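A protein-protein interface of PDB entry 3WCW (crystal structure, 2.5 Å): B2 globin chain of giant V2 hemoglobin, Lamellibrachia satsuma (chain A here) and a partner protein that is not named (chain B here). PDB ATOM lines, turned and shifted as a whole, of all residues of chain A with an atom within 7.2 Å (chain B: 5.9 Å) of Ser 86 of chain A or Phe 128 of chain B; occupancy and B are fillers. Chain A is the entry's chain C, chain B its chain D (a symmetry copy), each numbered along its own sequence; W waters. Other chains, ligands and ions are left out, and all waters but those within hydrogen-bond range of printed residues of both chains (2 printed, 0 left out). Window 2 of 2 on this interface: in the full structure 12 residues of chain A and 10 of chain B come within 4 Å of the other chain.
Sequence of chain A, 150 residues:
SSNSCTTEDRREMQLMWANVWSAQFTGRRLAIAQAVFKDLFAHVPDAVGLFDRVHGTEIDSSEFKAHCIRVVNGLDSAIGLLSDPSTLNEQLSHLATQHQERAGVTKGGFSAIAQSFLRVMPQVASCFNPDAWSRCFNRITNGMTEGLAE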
ATOM      1  N   LEU A  81     -14.873 -32.299  11.061  1.00  0.00           N
ATOM      2  CA  LEU A  81     -14.339 -30.956  10.952  1.00  0.00           C
ATOM      3  C   LEU A  81     -15.431 -29.882  10.898  1.00  0.00           C
ATOM      4  O   LEU A  81     -15.137 -28.687  10.861  1.00  0.00           O
ATOM      5  CB  LEU A  81     -13.385 -30.860   9.748  1.00  0.00           C
ATOM      6  CG  LEU A  81     -11.987 -31.433  10.061  1.00  0.00           C
ATOM      7  CD1 LEU A  81     -11.106 -31.449   8.833  1.00  0.00           C
ATOM      8  CD2 LEU A  81     -11.328 -30.590  11.155  1.00  0.00           C
ATOM      9  N   LEU A  82     -16.693 -30.295  10.917  1.00  0.00           N
ATOM     10  CA  LEU A  82     -17.774 -29.309  10.914  1.00  0.00           C
ATOM     11  C   LEU A  82     -17.682 -28.471  12.204  1.00  0.00           C
ATOM     12  O   LEU A  82     -18.192 -27.357  12.264  1.00  0.00           O
ATOM     13  CB  LEU A  82     -19.132 -30.010  10.819  1.00  0.00           C
ATOM     14  CG  LEU A  82     -19.437 -30.600   9.437  1.00  0.00           C
ATOM     15  CD1 LEU A  82     -20.628 -31.518   9.494  1.00  0.00           C
ATOM     16  CD2 LEU A  82     -19.696 -29.458   8.449  1.00  0.00           C
ATOM     17  N   SER A  83     -17.009 -29.017  13.219  1.00  0.00           N
ATOM     18  CA  SER A  83     -16.815 -28.346  14.504  1.00  0.00           C
ATOM     19  C   SER A  83     -15.702 -27.312  14.477  1.00  0.00           C
ATOM     20  O   SER A  83     -15.561 -26.540  15.419  1.00  0.00           O
ATOM     21  CB  SER A  83     -16.473 -29.358  15.595  1.00  0.00           C
ATOM     22  OG  SER A  83     -17.551 -30.230  15.843  1.00  0.00           O
ATOM     23  N   ASP A  84     -14.899 -27.316  13.415  1.00  0.00           N
ATOM     24  CA  ASP A  84     -13.796 -26.372  13.289  1.00  0.00           C
ATOM     25  C   ASP A  84     -13.691 -25.951  11.826  1.00  0.00           C
ATOM     26  O   ASP A  84     -12.780 -26.369  11.105  1.00  0.00           O
ATOM     27  CB  ASP A  84     -12.497 -27.028  13.764  1.00  0.00           C
ATOM     28  CG  ASP A  84     -11.318 -26.054  13.792  1.00  0.00           C
ATOM     29  OD1 ASP A  84     -11.454 -24.946  14.367  1.00  0.00           O
ATOM     30  OD2 ASP A  84     -10.244 -26.404  13.245  1.00  0.00           O
ATOM     31  N   PRO A  85     -14.633 -25.102  11.373  1.00  0.00           N
ATOM     32  CA  PRO A  85     -14.735 -24.577  10.009  1.00  0.00           C
ATOM     33  C   PRO A  85     -13.448 -24.043   9.379  1.00  0.00           C
ATOM     34  O   PRO A  85     -13.276 -24.137   8.161  1.00  0.00           O
ATOM     35  CB  PRO A  85     -15.813 -23.507  10.140  1.00  0.00           C
ATOM     36  CG  PRO A  85     -16.688 -24.063  11.199  1.00  0.00           C
ATOM     37  CD  PRO A  85     -15.685 -24.512  12.220  1.00  0.00           C
ATOM     38  N   SER A  86     -12.557 -23.474  10.190  1.00  0.00           N
ATOM     39  CA  SER A  86     -11.291 -22.946   9.672  1.00  0.00           C
ATOM     40  C   SER A  86     -10.517 -24.039   8.955  1.00  0.00           C
ATOM     41  O   SER A  86     -10.161 -23.911   7.787  1.00  0.00           O
ATOM     42  CB  SER A  86     -10.427 -22.408  10.805  1.00  0.00           C
ATOM     43  OG  SER A  86     -10.776 -21.081  11.118  1.00  0.00           O
ATOM     44  N   THR A  87     -10.257 -25.115   9.681  1.00  0.00           N
ATOM     45  CA  THR A  87      -9.530 -26.247   9.146  1.00  0.00           C
ATOM     46  C   THR A  87     -10.372 -26.913   8.060  1.00  0.00           C
ATOM     47  O   THR A  87      -9.854 -27.296   7.002  1.00  0.00           O
ATOM     48  CB  THR A  87      -9.216 -27.244  10.269  1.00  0.00           C
ATOM     49  OG1 THR A  87      -8.585 -26.541  11.345  1.00  0.00           O
ATOM     50  CG2 THR A  87      -8.293 -28.349   9.782  1.00  0.00           C
ATOM     51  N   LEU A  88     -11.673 -27.033   8.317  1.00  0.00           N
ATOM     52  CA  LEU A  88     -12.581 -27.641   7.349  1.00  0.00           C
ATOM     53  C   LEU A  88     -12.389 -27.017   5.971  1.00  0.00           C
ATOM     54  O   LEU A  88     -12.272 -27.726   4.971  1.00  0.00           O
ATOM     55  CB  LEU A  88     -14.043 -27.466   7.780  1.00  0.00           C
ATOM     56  CG  LEU A  88     -15.100 -27.847   6.734  1.00  0.00           C
ATOM     57  CD1 LEU A  88     -15.126 -29.364   6.525  1.00  0.00           C
ATOM     58  CD2 LEU A  88     -16.460 -27.353   7.192  1.00  0.00           C
ATOM     59  N   ASN A  89     -12.363 -25.688   5.915  1.00  0.00           N
ATOM     60  CA  ASN A  89     -12.199 -25.017   4.637  1.00  0.00           C
ATOM     61  C   ASN A  89     -10.927 -25.469   3.942  1.00  0.00           C
ATOM     62  O   ASN A  89     -10.927 -25.702   2.740  1.00  0.00           O
ATOM     63  CB  ASN A  89     -12.235 -23.497   4.812  1.00  0.00           C
ATOM     64  CG  ASN A  89     -13.623 -23.003   5.144  1.00  0.00           C
ATOM     65  OD1 ASN A  89     -14.607 -23.571   4.668  1.00  0.00           O
ATOM     66  ND2 ASN A  89     -13.718 -21.945   5.962  1.00  0.00           N
ATOM     67  N   GLU A  90      -9.849 -25.612   4.698  1.00  0.00           N
ATOM     68  CA  GLU A  90      -8.601 -26.076   4.113  1.00  0.00           C
ATOM     69  C   GLU A  90      -8.804 -27.499   3.584  1.00  0.00           C
ATOM     70  O   GLU A  90      -8.554 -27.783   2.409  1.00  0.00           O
ATOM     71  CB  GLU A  90      -7.489 -26.040   5.158  1.00  0.00           C
ATOM     72  CG  GLU A  90      -7.077 -24.636   5.529  1.00  0.00           C
ATOM     73  CD  GLU A  90      -6.561 -23.873   4.320  1.00  0.00           C
ATOM     74  OE1 GLU A  90      -5.476 -24.239   3.803  1.00  0.00           O
ATOM     75  OE2 GLU A  90      -7.248 -22.919   3.875  1.00  0.00           O
ATOM     76  N   GLN A  91      -9.278 -28.386   4.450  1.00  0.00           N
ATOM     77  CA  GLN A  91      -9.514 -29.769   4.068  1.00  0.00           C
ATOM     78  C   GLN A  91     -10.409 -29.842   2.829  1.00  0.00           C
ATOM     79  O   GLN A  91     -10.181 -30.642   1.935  1.00  0.00           O
ATOM     80  CB  GLN A  91     -10.160 -30.525   5.234  1.00  0.00           C
ATOM     81  CG  GLN A  91     -10.481 -31.972   4.935  1.00  0.00           C
ATOM     82  CD  GLN A  91      -9.238 -32.827   4.804  1.00  0.00           C
ATOM     83  OE1 GLN A  91      -8.271 -32.455   4.125  1.00  0.00           O
ATOM     84  NE2 GLN A  91      -9.256 -33.987   5.456  1.00  0.00           N
ATOM     85  N   ARG A 139     -23.313 -28.225   2.573  1.00  0.00           N
ATOM     86  CA  ARG A 139     -22.302 -27.289   3.040  1.00  0.00           C
ATOM     87  C   ARG A 139     -20.967 -27.924   2.696  1.00  0.00           C
ATOM     88  O   ARG A 139     -20.077 -27.266   2.155  1.00  0.00           O
ATOM     89  CB  ARG A 139     -22.400 -27.095   4.564  1.00  0.00           C
ATOM     90  CG  ARG A 139     -21.084 -26.686   5.243  1.00  0.00           C
ATOM     91  CD  ARG A 139     -20.642 -25.303   4.802  1.00  0.00           C
ATOM     92  NE  ARG A 139     -19.414 -24.863   5.460  1.00  0.00           N
ATOM     93  CZ  ARG A 139     -18.221 -24.809   4.872  1.00  0.00           C
ATOM     94  NH1 ARG A 139     -18.078 -25.175   3.605  1.00  0.00           N
ATOM     95  NH2 ARG A 139     -17.174 -24.357   5.544  1.00  0.00           N
ATOM     96  N   GLN B  15     -17.487 -14.940  20.647  1.00  0.00           N
ATOM     97  CA  GLN B  15     -16.204 -14.624  20.021  1.00  0.00           C
ATOM     98  C   GLN B  15     -16.010 -13.120  19.904  1.00  0.00           C
ATOM     99  O   GLN B  15     -14.897 -12.604  20.064  1.00  0.00           O
ATOM    100  CB  GLN B  15     -16.092 -15.270  18.635  1.00  0.00           C
ATOM    101  CG  GLN B  15     -16.216 -16.790  18.638  1.00  0.00           C
ATOM    102  CD  GLN B  15     -15.708 -17.434  17.344  1.00  0.00           C
ATOM    103  OE1 GLN B  15     -15.962 -16.944  16.235  1.00  0.00           O
ATOM    104  NE2 GLN B  15     -14.995 -18.546  17.487  1.00  0.00           N
ATOM    105  N   LEU B 117     -14.420  -8.109   7.079  1.00  0.00           N
ATOM    106  CA  LEU B 117     -14.608  -8.611   8.424  1.00  0.00           C
ATOM    107  C   LEU B 117     -14.144 -10.065   8.492  1.00  0.00           C
ATOM    108  O   LEU B 117     -13.397 -10.439   9.401  1.00  0.00           O
ATOM    109  CB  LEU B 117     -16.074  -8.473   8.853  1.00  0.00           C
ATOM    110  CG  LEU B 117     -16.514  -7.015   9.054  1.00  0.00           C
ATOM    111  CD1 LEU B 117     -17.993  -6.949   9.393  1.00  0.00           C
ATOM    112  CD2 LEU B 117     -15.685  -6.380  10.159  1.00  0.00           C
ATOM    113  N   MET B 118     -14.559 -10.875   7.520  1.00  0.00           N
ATOM    114  CA  MET B 118     -14.184 -12.289   7.503  1.00  0.00           C
ATOM    115  C   MET B 118     -12.682 -12.506   7.348  1.00  0.00           C
ATOM    116  O   MET B 118     -12.179 -13.606   7.581  1.00  0.00           O
ATOM    117  CB  MET B 118     -14.915 -13.020   6.377  1.00  0.00           C
ATOM    118  CG  MET B 118     -16.416 -13.049   6.521  1.00  0.00           C
ATOM    119  SD  MET B 118     -16.976 -13.893   8.017  1.00  0.00           S
ATOM    120  CE  MET B 118     -16.352 -15.517   7.766  1.00  0.00           C
ATOM    121  N   LEU B 121     -11.252 -10.379  11.370  1.00  0.00           N
ATOM    122  CA  LEU B 121     -11.645 -11.022  12.625  1.00  0.00           C
ATOM    123  C   LEU B 121     -10.805 -12.257  13.008  1.00  0.00           C
ATOM    124  O   LEU B 121     -10.432 -12.419  14.179  1.00  0.00           O
ATOM    125  CB  LEU B 121     -13.143 -11.358  12.605  1.00  0.00           C
ATOM    126  CG  LEU B 121     -14.057 -10.120  12.579  1.00  0.00           C
ATOM    127  CD1 LEU B 121     -15.501 -10.550  12.577  1.00  0.00           C
ATOM    128  CD2 LEU B 121     -13.785  -9.231  13.793  1.00  0.00           C
ATOM    129  N   PRO B 122     -10.491 -13.140  12.037  1.00  0.00           N
ATOM    130  CA  PRO B 122      -9.686 -14.312  12.396  1.00  0.00           C
ATOM    131  C   PRO B 122      -8.316 -13.942  12.953  1.00  0.00           C
ATOM    132  O   PRO B 122      -7.756 -14.666  13.773  1.00  0.00           O
ATOM    133  CB  PRO B 122      -9.609 -15.108  11.086  1.00  0.00           C
ATOM    134  CG  PRO B 122      -9.855 -14.087  10.036  1.00  0.00           C
ATOM    135  CD  PRO B 122     -10.932 -13.226  10.635  1.00  0.00           C
ATOM    136  N   ILE B 125      -9.644 -12.896  16.689  1.00  0.00           N
ATOM    137  CA  ILE B 125     -10.348 -13.853  17.527  1.00  0.00           C
ATOM    138  C   ILE B 125      -9.724 -15.257  17.607  1.00  0.00           C
ATOM    139  O   ILE B 125      -9.162 -15.761  16.626  1.00  0.00           O
ATOM    140  CB  ILE B 125     -11.822 -13.948  17.039  1.00  0.00           C
ATOM    141  CG1 ILE B 125     -12.482 -12.566  17.160  1.00  0.00           C
ATOM    142  CG2 ILE B 125     -12.598 -14.978  17.838  1.00  0.00           C
ATOM    143  CD1 ILE B 125     -13.825 -12.448  16.448  1.00  0.00           C
ATOM    144  N   ASP B 126      -9.823 -15.865  18.795  1.00  0.00           N
ATOM    145  CA  ASP B 126      -9.325 -17.215  19.054  1.00  0.00           C
ATOM    146  C   ASP B 126     -10.309 -18.235  18.491  1.00  0.00           C
ATOM    147  O   ASP B 126     -11.495 -18.241  18.864  1.00  0.00           O
ATOM    148  CB  ASP B 126      -9.191 -17.471  20.556  1.00  0.00           C
ATOM    149  CG  ASP B 126      -8.030 -16.740  21.175  1.00  0.00           C
ATOM    150  OD1 ASP B 126      -7.215 -16.167  20.427  1.00  0.00           O
ATOM    151  OD2 ASP B 126      -7.927 -16.745  22.420  1.00  0.00           O
ATOM    152  N   ASN B 127      -9.813 -19.107  17.614  1.00  0.00           N
ATOM    153  CA  ASN B 127     -10.641 -20.139  16.991  1.00  0.00           C
ATOM    154  C   ASN B 127     -11.826 -19.569  16.266  1.00  0.00           C
ATOM    155  O   ASN B 127     -12.937 -20.072  16.388  1.00  0.00           O
ATOM    156  CB  ASN B 127     -11.151 -21.139  18.025  1.00  0.00           C
ATOM    157  CG  ASN B 127     -10.210 -22.306  18.208  1.00  0.00           C
ATOM    158  OD1 ASN B 127      -9.973 -23.087  17.273  1.00  0.00           O
ATOM    159  ND2 ASN B 127      -9.664 -22.436  19.414  1.00  0.00           N
ATOM    160  N   PHE B 128     -11.583 -18.510  15.510  1.00  0.00           N
ATOM    161  CA  PHE B 128     -12.616 -17.845  14.738  1.00  0.00           C
ATOM    162  C   PHE B 128     -13.449 -18.873  13.990  1.00  0.00           C
ATOM    163  O   PHE B 128     -12.892 -19.757  13.337  1.00  0.00           O
ATOM    164  CB  PHE B 128     -11.965 -16.901  13.726  1.00  0.00           C
ATOM    165  CG  PHE B 128     -12.941 -16.240  12.797  1.00  0.00           C
ATOM    166  CD1 PHE B 128     -13.819 -15.265  13.270  1.00  0.00           C
ATOM    167  CD2 PHE B 128     -12.976 -16.585  11.445  1.00  0.00           C
ATOM    168  CE1 PHE B 128     -14.709 -14.646  12.418  1.00  0.00           C
ATOM    169  CE2 PHE B 128     -13.868 -15.961  10.584  1.00  0.00           C
ATOM    170  CZ  PHE B 128     -14.739 -14.987  11.073  1.00  0.00           C
ATOM    171  N   ASN B 129     -14.772 -18.757  14.075  1.00  0.00           N
ATOM    172  CA  ASN B 129     -15.650 -19.680  13.366  1.00  0.00           C
ATOM    173  C   ASN B 129     -16.257 -19.031  12.112  1.00  0.00           C
ATOM    174  O   ASN B 129     -17.366 -18.502  12.147  1.00  0.00           O
ATOM    175  CB  ASN B 129     -16.770 -20.156  14.288  1.00  0.00           C
ATOM    176  CG  ASN B 129     -17.533 -21.335  13.710  1.00  0.00           C
ATOM    177  OD1 ASN B 129     -17.728 -21.426  12.491  1.00  0.00           O
ATOM    178  ND2 ASN B 129     -17.977 -22.241  14.582  1.00  0.00           N
ATOM    179  N   PRO B 130     -15.547 -19.092  10.980  1.00  0.00           N
ATOM    180  CA  PRO B 130     -16.064 -18.490   9.746  1.00  0.00           C
ATOM    181  C   PRO B 130     -17.476 -18.928   9.344  1.00  0.00           C
ATOM    182  O   PRO B 130     -18.201 -18.169   8.705  1.00  0.00           O
ATOM    183  CB  PRO B 130     -15.009 -18.879   8.707  1.00  0.00           C
ATOM    184  CG  PRO B 130     -14.503 -20.195   9.222  1.00  0.00           C
ATOM    185  CD  PRO B 130     -14.361 -19.925  10.703  1.00  0.00           C
ATOM    186  N   ASP B 131     -17.871 -20.143   9.710  1.00  0.00           N
ATOM    187  CA  ASP B 131     -19.205 -20.636   9.358  1.00  0.00           C
ATOM    188  C   ASP B 131     -20.317 -20.038  10.193  1.00  0.00           C
ATOM    189  O   ASP B 131     -21.354 -19.643   9.661  1.00  0.00           O
ATOM    190  CB  ASP B 131     -19.274 -22.160   9.464  1.00  0.00           C
ATOM    191  CG  ASP B 131     -18.792 -22.844   8.211  1.00  0.00           C
ATOM    192  OD1 ASP B 131     -18.974 -24.077   8.098  1.00  0.00           O
ATOM    193  OD2 ASP B 131     -18.232 -22.143   7.336  1.00  0.00           O
ATOM    194  N   TRP B 133     -20.128 -17.276  11.734  1.00  0.00           N
ATOM    195  CA  TRP B 133     -20.149 -15.843  11.451  1.00  0.00           C
ATOM    196  C   TRP B 133     -20.845 -15.580  10.141  1.00  0.00           C
ATOM    197  O   TRP B 133     -21.700 -14.705  10.049  1.00  0.00           O
ATOM    198  CB  TRP B 133     -18.735 -15.259  11.423  1.00  0.00           C
ATOM    199  CG  TRP B 133     -18.210 -14.937  12.801  1.00  0.00           C
ATOM    200  CD1 TRP B 133     -17.659 -15.810  13.698  1.00  0.00           C
ATOM    201  CD2 TRP B 133     -18.240 -13.661  13.450  1.00  0.00           C
ATOM    202  NE1 TRP B 133     -17.343 -15.153  14.866  1.00  0.00           N
ATOM    203  CE2 TRP B 133     -17.689 -13.835  14.741  1.00  0.00           C
ATOM    204  CE3 TRP B 133     -18.681 -12.389  13.070  1.00  0.00           C
ATOM    205  CZ2 TRP B 133     -17.568 -12.781  15.652  1.00  0.00           C
ATOM    206  CZ3 TRP B 133     -18.562 -11.338  13.980  1.00  0.00           C
ATOM    207  CH2 TRP B 133     -18.006 -11.546  15.258  1.00  0.00           C
HETATM  208  O   HOH W   1     -13.162 -22.683  13.085  1.00  0.00           O
HETATM  209  O   HOH W   2     -16.354 -21.118   5.509  1.00  0.00           O
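Water W2 lies within hydrogen-bond range of ND2 of Asn 89 of chain A (2.8 Å), OD2 of Asp 131 of chain B (2.8 Å) and NH2 of Arg 139 of chain A (3.3 Å).
Water W1 lies within hydrogen-bond range of O of Phe 128 of chain B, N of Ser 86 of chain A and OD1 of Asp 84 of chain A.
Ser 86 of chain A touches just these residues of chain B: Phe 128 (3.3 Å) and Pro 130 (3.8 Å).
Thr 87 of chain A touches none of the printed residues of chain B.
Of the printed residues of chain B, Arg 139 of chain A touches Asp 131.
Of the printed residues of chain A, Asn 127 of chain B touches Asp 84.
Phe 128 of chain B touches just one residue of chain A: Ser 86 (3.3 Å).
Trp 133 of chain B touches none of the printed residues of chain A.
The nearest residue of chain A that does not touch Phe 128 of chain B is Asp 84 of chain A (5.5 Å).
Of the 13 printed residues of chain B, 5 touch a printed residue of chain A.
Hydrophobic or aromatic side chains of chain B that line the printed part of chain A: Pro 130.
Hydrophobic or aromatic side chains of chain A within 4 Å of the printed part of chain B: Pro 85.
Among the printed residues, Asp or Glu carboxylates within 4 Å of a Lys or Arg side-chain nitrogen of the other chain: Arg 139 of chain A with Asp 131 of chain B (2.8 Å).
The guanidinium group (NH2) of Arg 139 of chain A lies within hydrogen-bond range of the side-chain amide oxygen (OD1) of Asn 89 of chain A (2.8 Å).
N of Asp 131 of chain B is in hydrogen-bond range of OD1 of Asn 129 of chain B.
The side-chain amide nitrogen of Gln 15 of chain B is in hydrogen-bond range of the backbone carbonyl oxygen of Asn 127 of chain B, 2.8 Å away.
The side-chain hydroxyl (OG1) of Thr 87 of chain A is in hydrogen-bond range of the side-chain carboxylate (OD2) of Asp 84 of chain A, at 2.5 Å.
ND2 of Asn 89 of chain A sits at hydrogen-bond distance from O of Pro 85 of chain A (3.1 Å).
The side-chain amide oxygen (OE1) of Gln 15 of chain B is in hydrogen-bond range of the backbone NH (N) of Asn 129 of chain B, at 3.1 Å.
Asn 127 of chain B touches Asp 84 of chain A.
Pro 85 of chain A touches Asn 129 of chain B.
Pro 85 of chain A touches Pro 130 of chain B.
CG of Asp 131 of chain B touches CB of Pro 85 of chain A, at 3.6 Å.
Ser 86 of chain A touches Pro 130 of chain B.
Asn 89 of chain A touches Pro 130 of chain B (ND2 to CG, 3.8 Å).
OG of Ser 86 of chain A lies within hydrogen-bond range of O of Phe 128 of chain B (3.3 Å).
The guanidinium group (NE) of Arg 139 of chain A is in salt-bridge range of the side-chain carboxylate (OD1) of Asp 131 of chain B, at 2.8 Å.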
